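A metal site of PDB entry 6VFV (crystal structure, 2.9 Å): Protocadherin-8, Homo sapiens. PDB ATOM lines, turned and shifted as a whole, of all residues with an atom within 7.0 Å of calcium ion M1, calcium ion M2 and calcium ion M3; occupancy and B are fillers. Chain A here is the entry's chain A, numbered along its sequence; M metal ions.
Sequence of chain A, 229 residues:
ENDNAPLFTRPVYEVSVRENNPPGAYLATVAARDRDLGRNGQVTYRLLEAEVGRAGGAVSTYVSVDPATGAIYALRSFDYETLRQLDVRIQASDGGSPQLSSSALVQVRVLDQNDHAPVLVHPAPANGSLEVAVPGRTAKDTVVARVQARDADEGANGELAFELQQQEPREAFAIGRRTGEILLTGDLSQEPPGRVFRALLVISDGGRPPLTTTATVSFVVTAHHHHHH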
ATOM      1  N   GLU A  19      -9.454  11.487 -26.101  1.00  0.00           N
ATOM      2  CA  GLU A  19      -9.568  11.613 -27.548  1.00  0.00           C
ATOM      3  C   GLU A  19     -10.817  10.912 -28.070  1.00  0.00           C
ATOM      4  O   GLU A  19     -11.347   9.978 -27.454  1.00  0.00           O
ATOM      5  CB  GLU A  19      -8.305  11.024 -28.190  1.00  0.00           C
ATOM      6  CG  GLU A  19      -8.214  11.120 -29.688  1.00  0.00           C
ATOM      7  CD  GLU A  19      -7.016  10.352 -30.223  1.00  0.00           C
ATOM      8  OE1 GLU A  19      -6.322   9.697 -29.413  1.00  0.00           O
ATOM      9  OE2 GLU A  19      -6.773  10.412 -31.445  1.00  0.00           O
ATOM     10  N   ASN A  20     -11.293  11.370 -29.226  1.00  0.00           N
ATOM     11  CA  ASN A  20     -12.431  10.764 -29.926  1.00  0.00           C
ATOM     12  C   ASN A  20     -13.702  10.821 -29.073  1.00  0.00           C
ATOM     13  O   ASN A  20     -14.448   9.839 -28.957  1.00  0.00           O
ATOM     14  CB  ASN A  20     -12.115   9.326 -30.343  1.00  0.00           C
ATOM     15  CG  ASN A  20     -10.814   9.219 -31.134  1.00  0.00           C
ATOM     16  OD1 ASN A  20     -10.563   9.999 -32.058  1.00  0.00           O
ATOM     17  ND2 ASN A  20      -9.979   8.263 -30.763  1.00  0.00           N
ATOM     18  N   PHE A  78     -12.272  15.252 -30.386  1.00  0.00           N
ATOM     19  CA  PHE A  78     -10.891  15.711 -30.335  1.00  0.00           C
ATOM     20  C   PHE A  78      -9.943  14.579 -30.725  1.00  0.00           C
ATOM     21  O   PHE A  78     -10.134  13.432 -30.325  1.00  0.00           O
ATOM     22  CB  PHE A  78     -10.544  16.226 -28.937  1.00  0.00           C
ATOM     23  CG  PHE A  78     -11.406  17.374 -28.483  1.00  0.00           C
ATOM     24  CD1 PHE A  78     -11.899  17.426 -27.193  1.00  0.00           C
ATOM     25  CD2 PHE A  78     -11.709  18.419 -29.354  1.00  0.00           C
ATOM     26  CE1 PHE A  78     -12.687  18.490 -26.780  1.00  0.00           C
ATOM     27  CE2 PHE A  78     -12.491  19.476 -28.941  1.00  0.00           C
ATOM     28  CZ  PHE A  78     -12.983  19.514 -27.655  1.00  0.00           C
ATOM     29  N   ASP A  79      -8.927  14.931 -31.504  1.00  0.00           N
ATOM     30  CA  ASP A  79      -7.896  13.997 -31.960  1.00  0.00           C
ATOM     31  C   ASP A  79      -6.571  14.365 -31.292  1.00  0.00           C
ATOM     32  O   ASP A  79      -6.032  15.448 -31.534  1.00  0.00           O
ATOM     33  CB  ASP A  79      -7.765  14.033 -33.481  1.00  0.00           C
ATOM     34  CG  ASP A  79      -6.627  13.170 -33.983  1.00  0.00           C
ATOM     35  OD1 ASP A  79      -6.201  12.259 -33.244  1.00  0.00           O
ATOM     36  OD2 ASP A  79      -6.180  13.395 -35.133  1.00  0.00           O
ATOM     37  N   TYR A  80      -6.066  13.466 -30.450  1.00  0.00           N
ATOM     38  CA  TYR A  80      -4.856  13.772 -29.683  1.00  0.00           C
ATOM     39  C   TYR A  80      -3.659  13.958 -30.607  1.00  0.00           C
ATOM     40  O   TYR A  80      -2.806  14.824 -30.363  1.00  0.00           O
ATOM     41  CB  TYR A  80      -4.586  12.662 -28.665  1.00  0.00           C
ATOM     42  CG  TYR A  80      -3.297  12.851 -27.891  1.00  0.00           C
ATOM     43  CD1 TYR A  80      -3.263  13.636 -26.751  1.00  0.00           C
ATOM     44  CD2 TYR A  80      -2.117  12.250 -28.304  1.00  0.00           C
ATOM     45  CE1 TYR A  80      -2.097  13.817 -26.039  1.00  0.00           C
ATOM     46  CE2 TYR A  80      -0.938  12.428 -27.611  1.00  0.00           C
ATOM     47  CZ  TYR A  80      -0.932  13.215 -26.478  1.00  0.00           C
ATOM     48  OH  TYR A  80       0.248  13.379 -25.787  1.00  0.00           O
ATOM     49  N   GLU A  81      -3.563  13.161 -31.667  1.00  0.00           N
ATOM     50  CA  GLU A  81      -2.460  13.314 -32.607  1.00  0.00           C
ATOM     51  C   GLU A  81      -2.509  14.659 -33.325  1.00  0.00           C
ATOM     52  O   GLU A  81      -1.509  15.089 -33.885  1.00  0.00           O
ATOM     53  CB  GLU A  81      -2.471  12.171 -33.624  1.00  0.00           C
ATOM     54  CG  GLU A  81      -2.005  10.825 -33.066  1.00  0.00           C
ATOM     55  CD  GLU A  81      -3.008  10.191 -32.116  1.00  0.00           C
ATOM     56  OE1 GLU A  81      -4.172   9.986 -32.521  1.00  0.00           O
ATOM     57  OE2 GLU A  81      -2.632   9.913 -30.958  1.00  0.00           O
ATOM     58  N   THR A  82      -3.662  15.334 -33.305  1.00  0.00           N
ATOM     59  CA  THR A  82      -3.845  16.627 -33.960  1.00  0.00           C
ATOM     60  C   THR A  82      -3.846  17.797 -32.994  1.00  0.00           C
ATOM     61  O   THR A  82      -3.545  18.922 -33.419  1.00  0.00           O
ATOM     62  CB  THR A  82      -5.171  16.608 -34.746  1.00  0.00           C
ATOM     63  OG1 THR A  82      -5.047  15.751 -35.887  1.00  0.00           O
ATOM     64  CG2 THR A  82      -5.581  18.012 -35.208  1.00  0.00           C
ATOM     65  N   LEU A 111      -6.500  13.716 -23.591  1.00  0.00           N
ATOM     66  CA  LEU A 111      -5.786  12.495 -23.269  1.00  0.00           C
ATOM     67  C   LEU A 111      -5.799  11.549 -24.465  1.00  0.00           C
ATOM     68  O   LEU A 111      -6.695  11.601 -25.314  1.00  0.00           O
ATOM     69  CB  LEU A 111      -6.404  11.796 -22.064  1.00  0.00           C
ATOM     70  CG  LEU A 111      -6.634  12.641 -20.819  1.00  0.00           C
ATOM     71  CD1 LEU A 111      -7.722  12.018 -19.979  1.00  0.00           C
ATOM     72  CD2 LEU A 111      -5.353  12.782 -20.027  1.00  0.00           C
ATOM     73  N   ASP A 112      -4.805  10.681 -24.506  1.00  0.00           N
ATOM     74  CA  ASP A 112      -4.639   9.769 -25.626  1.00  0.00           C
ATOM     75  C   ASP A 112      -5.539   8.549 -25.466  1.00  0.00           C
ATOM     76  O   ASP A 112      -5.846   8.095 -24.361  1.00  0.00           O
ATOM     77  CB  ASP A 112      -3.181   9.333 -25.749  1.00  0.00           C
ATOM     78  CG  ASP A 112      -2.941   8.431 -26.940  1.00  0.00           C
ATOM     79  OD1 ASP A 112      -3.655   8.577 -27.958  1.00  0.00           O
ATOM     80  OD2 ASP A 112      -2.033   7.571 -26.867  1.00  0.00           O
ATOM     81  N   GLN A 113      -5.979   8.028 -26.604  1.00  0.00           N
ATOM     82  CA  GLN A 113      -6.739   6.789 -26.718  1.00  0.00           C
ATOM     83  C   GLN A 113      -5.979   5.879 -27.672  1.00  0.00           C
ATOM     84  O   GLN A 113      -5.349   6.341 -28.620  1.00  0.00           O
ATOM     85  CB  GLN A 113      -8.157   7.081 -27.231  1.00  0.00           C
ATOM     86  CG  GLN A 113      -9.146   5.920 -27.256  1.00  0.00           C
ATOM     87  CD  GLN A 113     -10.524   6.346 -27.778  1.00  0.00           C
ATOM     88  OE1 GLN A 113     -10.760   7.527 -28.003  1.00  0.00           O
ATOM     89  NE2 GLN A 113     -11.410   5.384 -27.959  1.00  0.00           N
ATOM     90  N   ASN A 114      -5.999   4.570 -27.408  1.00  0.00           N
ATOM     91  CA  ASN A 114      -5.319   3.629 -28.299  1.00  0.00           C
ATOM     92  C   ASN A 114      -6.218   3.414 -29.517  1.00  0.00           C
ATOM     93  O   ASN A 114      -6.987   2.455 -29.617  1.00  0.00           O
ATOM     94  CB  ASN A 114      -4.995   2.321 -27.604  1.00  0.00           C
ATOM     95  CG  ASN A 114      -3.961   1.497 -28.365  1.00  0.00           C
ATOM     96  OD1 ASN A 114      -3.311   2.008 -29.273  1.00  0.00           O
ATOM     97  ND2 ASN A 114      -3.808   0.232 -28.004  1.00  0.00           N
ATOM     98  N   ASP A 115      -6.105   4.352 -30.467  1.00  0.00           N
ATOM     99  CA  ASP A 115      -6.912   4.347 -31.679  1.00  0.00           C
ATOM    100  C   ASP A 115      -6.030   4.154 -32.914  1.00  0.00           C
ATOM    101  O   ASP A 115      -6.361   4.628 -34.010  1.00  0.00           O
ATOM    102  CB  ASP A 115      -7.736   5.626 -31.795  1.00  0.00           C
ATOM    103  CG  ASP A 115      -6.883   6.864 -31.794  1.00  0.00           C
ATOM    104  OD1 ASP A 115      -5.771   6.823 -31.218  1.00  0.00           O
ATOM    105  OD2 ASP A 115      -7.313   7.887 -32.366  1.00  0.00           O
ATOM    106  N   HIS A 116      -4.899   3.480 -32.758  1.00  0.00           N
ATOM    107  CA  HIS A 116      -4.020   3.140 -33.868  1.00  0.00           C
ATOM    108  C   HIS A 116      -3.476   1.740 -33.655  1.00  0.00           C
ATOM    109  O   HIS A 116      -2.829   1.463 -32.637  1.00  0.00           O
ATOM    110  CB  HIS A 116      -2.868   4.143 -34.024  1.00  0.00           C
ATOM    111  CG  HIS A 116      -3.271   5.420 -34.687  1.00  0.00           C
ATOM    112  ND1 HIS A 116      -3.328   6.619 -34.022  1.00  0.00           N
ATOM    113  CD2 HIS A 116      -3.618   5.678 -35.970  1.00  0.00           C
ATOM    114  CE1 HIS A 116      -3.698   7.576 -34.860  1.00  0.00           C
ATOM    115  NE2 HIS A 116      -3.872   7.027 -36.052  1.00  0.00           N
ATOM    116  N   ALA A 117      -3.730   0.883 -34.570  1.00  0.00           N
ATOM    117  CA  ALA A 117      -3.046  -0.396 -34.551  1.00  0.00           C
ATOM    118  C   ALA A 117      -1.703  -0.268 -35.261  1.00  0.00           C
ATOM    119  O   ALA A 117      -1.552   0.557 -36.163  1.00  0.00           O
ATOM    120  CB  ALA A 117      -3.897  -1.459 -35.242  1.00  0.00           C
ATOM    121  N   PRO A 118      -0.700  -1.051 -34.870  1.00  0.00           N
ATOM    122  CA  PRO A 118       0.585  -0.978 -35.568  1.00  0.00           C
ATOM    123  C   PRO A 118       0.406  -1.244 -37.057  1.00  0.00           C
ATOM    124  O   PRO A 118      -0.409  -2.054 -37.469  1.00  0.00           O
ATOM    125  CB  PRO A 118       1.431  -2.058 -34.891  1.00  0.00           C
ATOM    126  CG  PRO A 118       0.454  -2.925 -34.151  1.00  0.00           C
ATOM    127  CD  PRO A 118      -0.687  -2.043 -33.786  1.00  0.00           C
ATOM    128  N   ASP A 151       3.542   3.027 -34.978  1.00  0.00           N
ATOM    129  CA  ASP A 151       2.321   3.223 -34.215  1.00  0.00           C
ATOM    130  C   ASP A 151       2.295   4.662 -33.729  1.00  0.00           C
ATOM    131  O   ASP A 151       3.253   5.122 -33.100  1.00  0.00           O
ATOM    132  CB  ASP A 151       2.248   2.251 -33.035  1.00  0.00           C
ATOM    133  CG  ASP A 151       0.871   2.213 -32.367  1.00  0.00           C
ATOM    134  OD1 ASP A 151       0.248   3.297 -32.210  1.00  0.00           O
ATOM    135  OD2 ASP A 151       0.413   1.116 -32.006  1.00  0.00           O
ATOM    136  N   ALA A 152       1.215   5.363 -34.025  1.00  0.00           N
ATOM    137  CA  ALA A 152       1.143   6.802 -33.779  1.00  0.00           C
ATOM    138  C   ALA A 152       0.817   7.155 -32.341  1.00  0.00           C
ATOM    139  O   ALA A 152       0.992   8.324 -31.966  1.00  0.00           O
ATOM    140  CB  ALA A 152       0.096   7.422 -34.698  1.00  0.00           C
ATOM    141  N   ASP A 153       0.361   6.204 -31.534  1.00  0.00           N
ATOM    142  CA  ASP A 153      -0.148   6.517 -30.207  1.00  0.00           C
ATOM    143  C   ASP A 153       1.005   6.835 -29.250  1.00  0.00           C
ATOM    144  O   ASP A 153       2.173   6.896 -29.632  1.00  0.00           O
ATOM    145  CB  ASP A 153      -1.013   5.361 -29.707  1.00  0.00           C
ATOM    146  CG  ASP A 153      -2.241   5.129 -30.570  1.00  0.00           C
ATOM    147  OD1 ASP A 153      -2.879   6.129 -30.998  1.00  0.00           O
ATOM    148  OD2 ASP A 153      -2.578   3.951 -30.826  1.00  0.00           O
ATOM    149  N   GLU A 154       0.655   7.047 -27.983  1.00  0.00           N
ATOM    150  CA  GLU A 154       1.585   7.514 -26.962  1.00  0.00           C
ATOM    151  C   GLU A 154       1.920   6.394 -25.992  1.00  0.00           C
ATOM    152  O   GLU A 154       1.198   5.408 -25.858  1.00  0.00           O
ATOM    153  CB  GLU A 154       0.977   8.709 -26.213  1.00  0.00           C
ATOM    154  CG  GLU A 154       1.758   9.170 -24.993  1.00  0.00           C
ATOM    155  CD  GLU A 154       1.219  10.462 -24.403  1.00  0.00           C
ATOM    156  OE1 GLU A 154       0.126  10.885 -24.814  1.00  0.00           O
ATOM    157  OE2 GLU A 154       1.891  11.038 -23.512  1.00  0.00           O
ATOM    158  N   ALA A 156       2.953   3.294 -23.911  1.00  0.00           N
ATOM    159  CA  ALA A 156       2.886   1.883 -24.280  1.00  0.00           C
ATOM    160  C   ALA A 156       1.991   1.659 -25.488  1.00  0.00           C
ATOM    161  O   ALA A 156       2.190   0.685 -26.236  1.00  0.00           O
ATOM    162  CB  ALA A 156       2.384   1.044 -23.094  1.00  0.00           C
ATOM    163  N   ASN A 157       1.007   2.535 -25.721  1.00  0.00           N
ATOM    164  CA  ASN A 157       0.170   2.408 -26.909  1.00  0.00           C
ATOM    165  C   ASN A 157       0.956   2.520 -28.206  1.00  0.00           C
ATOM    166  O   ASN A 157       0.412   2.220 -29.269  1.00  0.00           O
ATOM    167  CB  ASN A 157      -0.941   3.464 -26.901  1.00  0.00           C
ATOM    168  CG  ASN A 157      -1.964   3.231 -25.804  1.00  0.00           C
ATOM    169  OD1 ASN A 157      -2.295   2.086 -25.479  1.00  0.00           O
ATOM    170  ND2 ASN A 157      -2.479   4.311 -25.237  1.00  0.00           N
ATOM    171  N   GLY A 158       2.208   2.955 -28.148  1.00  0.00           N
ATOM    172  CA  GLY A 158       3.075   2.971 -29.314  1.00  0.00           C
ATOM    173  C   GLY A 158       4.275   2.060 -29.141  1.00  0.00           C
ATOM    174  O   GLY A 158       5.138   1.977 -30.020  1.00  0.00           O
ATOM    175  N   GLU A 159       4.334   1.362 -28.002  1.00  0.00           N
ATOM    176  CA  GLU A 159       5.432   0.443 -27.711  1.00  0.00           C
ATOM    177  C   GLU A 159       5.154  -0.892 -28.396  1.00  0.00           C
ATOM    178  O   GLU A 159       4.254  -1.633 -27.989  1.00  0.00           O
ATOM    179  CB  GLU A 159       5.584   0.274 -26.198  1.00  0.00           C
ATOM    180  CG  GLU A 159       6.827  -0.460 -25.762  1.00  0.00           C
ATOM    181  CD  GLU A 159       7.012  -0.448 -24.248  1.00  0.00           C
ATOM    182  OE1 GLU A 159       6.068  -0.050 -23.531  1.00  0.00           O
ATOM    183  OE2 GLU A 159       8.106  -0.840 -23.786  1.00  0.00           O
ATOM    184  N   LEU A 160       5.926  -1.206 -29.437  1.00  0.00           N
ATOM    185  CA  LEU A 160       5.664  -2.356 -30.287  1.00  0.00           C
ATOM    186  C   LEU A 160       6.473  -3.579 -29.860  1.00  0.00           C
ATOM    187  O   LEU A 160       7.527  -3.480 -29.236  1.00  0.00           O
ATOM    188  CB  LEU A 160       5.972  -2.027 -31.746  1.00  0.00           C
ATOM    189  CG  LEU A 160       5.077  -0.965 -32.411  1.00  0.00           C
ATOM    190  CD1 LEU A 160       5.168  -1.090 -33.931  1.00  0.00           C
ATOM    191  CD2 LEU A 160       3.623  -1.071 -31.946  1.00  0.00           C
ATOM    192  N   ASP A 205       1.064  -3.889 -29.858  1.00  0.00           N
ATOM    193  CA  ASP A 205       1.401  -2.687 -29.101  1.00  0.00           C
ATOM    194  C   ASP A 205       1.068  -2.915 -27.636  1.00  0.00           C
ATOM    195  O   ASP A 205       0.506  -3.944 -27.258  1.00  0.00           O
ATOM    196  CB  ASP A 205       0.679  -1.457 -29.671  1.00  0.00           C
ATOM    197  CG  ASP A 205      -0.795  -1.408 -29.303  1.00  0.00           C
ATOM    198  OD1 ASP A 205      -1.327  -2.403 -28.768  1.00  0.00           O
ATOM    199  OD2 ASP A 205      -1.424  -0.366 -29.578  1.00  0.00           O
ATOM    200  N   GLY A 206       1.433  -1.944 -26.798  1.00  0.00           N
ATOM    201  CA  GLY A 206       1.348  -2.147 -25.367  1.00  0.00           C
ATOM    202  C   GLY A 206       0.052  -1.672 -24.742  1.00  0.00           C
ATOM    203  O   GLY A 206       0.037  -1.247 -23.587  1.00  0.00           O
ATOM    204  N   GLY A 207      -1.042  -1.732 -25.498  1.00  0.00           N
ATOM    205  CA  GLY A 207      -2.333  -1.326 -24.975  1.00  0.00           C
ATOM    206  C   GLY A 207      -2.956  -2.374 -24.072  1.00  0.00           C
ATOM    207  O   GLY A 207      -2.495  -3.513 -23.949  1.00  0.00           O
ATOM    208  N   LEU A 211      -3.656  -3.724 -29.415  1.00  0.00           N
ATOM    209  CA  LEU A 211      -4.049  -3.788 -30.813  1.00  0.00           C
ATOM    210  C   LEU A 211      -2.974  -4.533 -31.596  1.00  0.00           C
ATOM    211  O   LEU A 211      -1.796  -4.193 -31.509  1.00  0.00           O
ATOM    212  CB  LEU A 211      -4.277  -2.398 -31.393  1.00  0.00           C
ATOM    213  CG  LEU A 211      -5.485  -1.625 -30.850  1.00  0.00           C
ATOM    214  CD1 LEU A 211      -5.815  -0.456 -31.753  1.00  0.00           C
ATOM    215  CD2 LEU A 211      -6.718  -2.513 -30.692  1.00  0.00           C
HETATM  216 CA    CA M   1      -6.575  10.071 -33.567  1.00  0.00          CA
HETATM  217 CA    CA M   2      -4.237   8.012 -30.088  1.00  0.00          CA
HETATM  218 CA    CA M   3      -1.470   1.692 -30.679  1.00  0.00          CA
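Calcium ion M1 is bound by the side-chain carboxylate of Glu 19 (2.2 Å), the side-chain carboxylate of Asp 79 (2.2 Å), the side-chain carboxylate of Asp 115 (2.6 Å) and the side-chain carboxylate of Glu 81 (2.6 Å).
Calcium ion M1 has four donor atoms within binding distance.
Calcium ion M2 is bound by the side-chain carboxylate (OD1) of Asp 115 (2.2 Å), the side-chain carboxylate (OD1) of Asp 112 (2.3 Å), the backbone carbonyl oxygen (O) of Gln 113 (2.5 Å), the side-chain carboxylate (OD1) of Asp 153 (2.5 Å), the side-chain carboxylate (OE2) of Glu 81 (2.6 Å) and the side-chain carboxylate (OE1) of Glu 19 (2.8 Å).
Calcium ion M2 has six donor atoms within binding distance.
Slightly farther from calcium ion M2 lies the side-chain carboxylate (OE1) of Glu 81 (3.1 Å).
The side-chain carboxylate (OD2) of Asp 205 binds calcium ion M3 (2.3 Å).
Calcium ion M3 is bound by the side-chain amide oxygen (OD1) of Asn 114 (2.3 Å).
OD2 of Asp 151 binds calcium ion M3 (2.4 Å).
O of His 116 is bound to calcium ion M3, 2.4 Å away.
The backbone carbonyl oxygen (O) of Asn 157 is bound to calcium ion M3.
OD2 of Asp 153 binds calcium ion M3 (2.5 Å).
Calcium ion M3 is bound by OD1 of Asp 151, 2.8 Å away.
Within 4 Å of calcium ion M3: Asn 114, His 116, Asp 151, Asp 153, Asn 157 and Asp 205.
The nearest printed residue that does not touch calcium ion M3 is Ala 117 (4.6 Å).
Six residues have an atom within 4 Å of calcium ion M2: Glu 19, Glu 81, Asp 112, Gln 113, Asp 115 and Asp 153.
The nearest printed residue that does not touch calcium ion M2 is His 116 (4.3 Å).
N of Leu 211 lies within hydrogen-bond range of OD1 of Asp 205, 2.8 Å away.
OD2 of Asp 112 sits at hydrogen-bond distance from N of Glu 154 (3.0 Å).
The side-chain carboxylate (OD1) of Asp 205 lies close to the backbone NH (N) of Gly 207.
ND2 of Asn 20 sits close to OD2 of Asp 115 (3.1 Å).
OE1 of Gln 113 is in hydrogen-bond range of ND2 of Asn 20 (3.0 Å).
The side-chain hydroxyl (OG1) of Thr 82 lies within hydrogen-bond range of the side-chain carboxylate (OD2) of Asp 79, 2.7 Å away.
N of Tyr 80 lies close to OE2 of Glu 19.
The backbone NH (N) of Glu 19 lies within hydrogen-bond range of the backbone carbonyl oxygen (O) of Leu 111, 2.9 Å away.
Four residues have an atom within 4 Å of calcium ion M1: Glu 19, Asp 79, Glu 81 and Asp 115.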
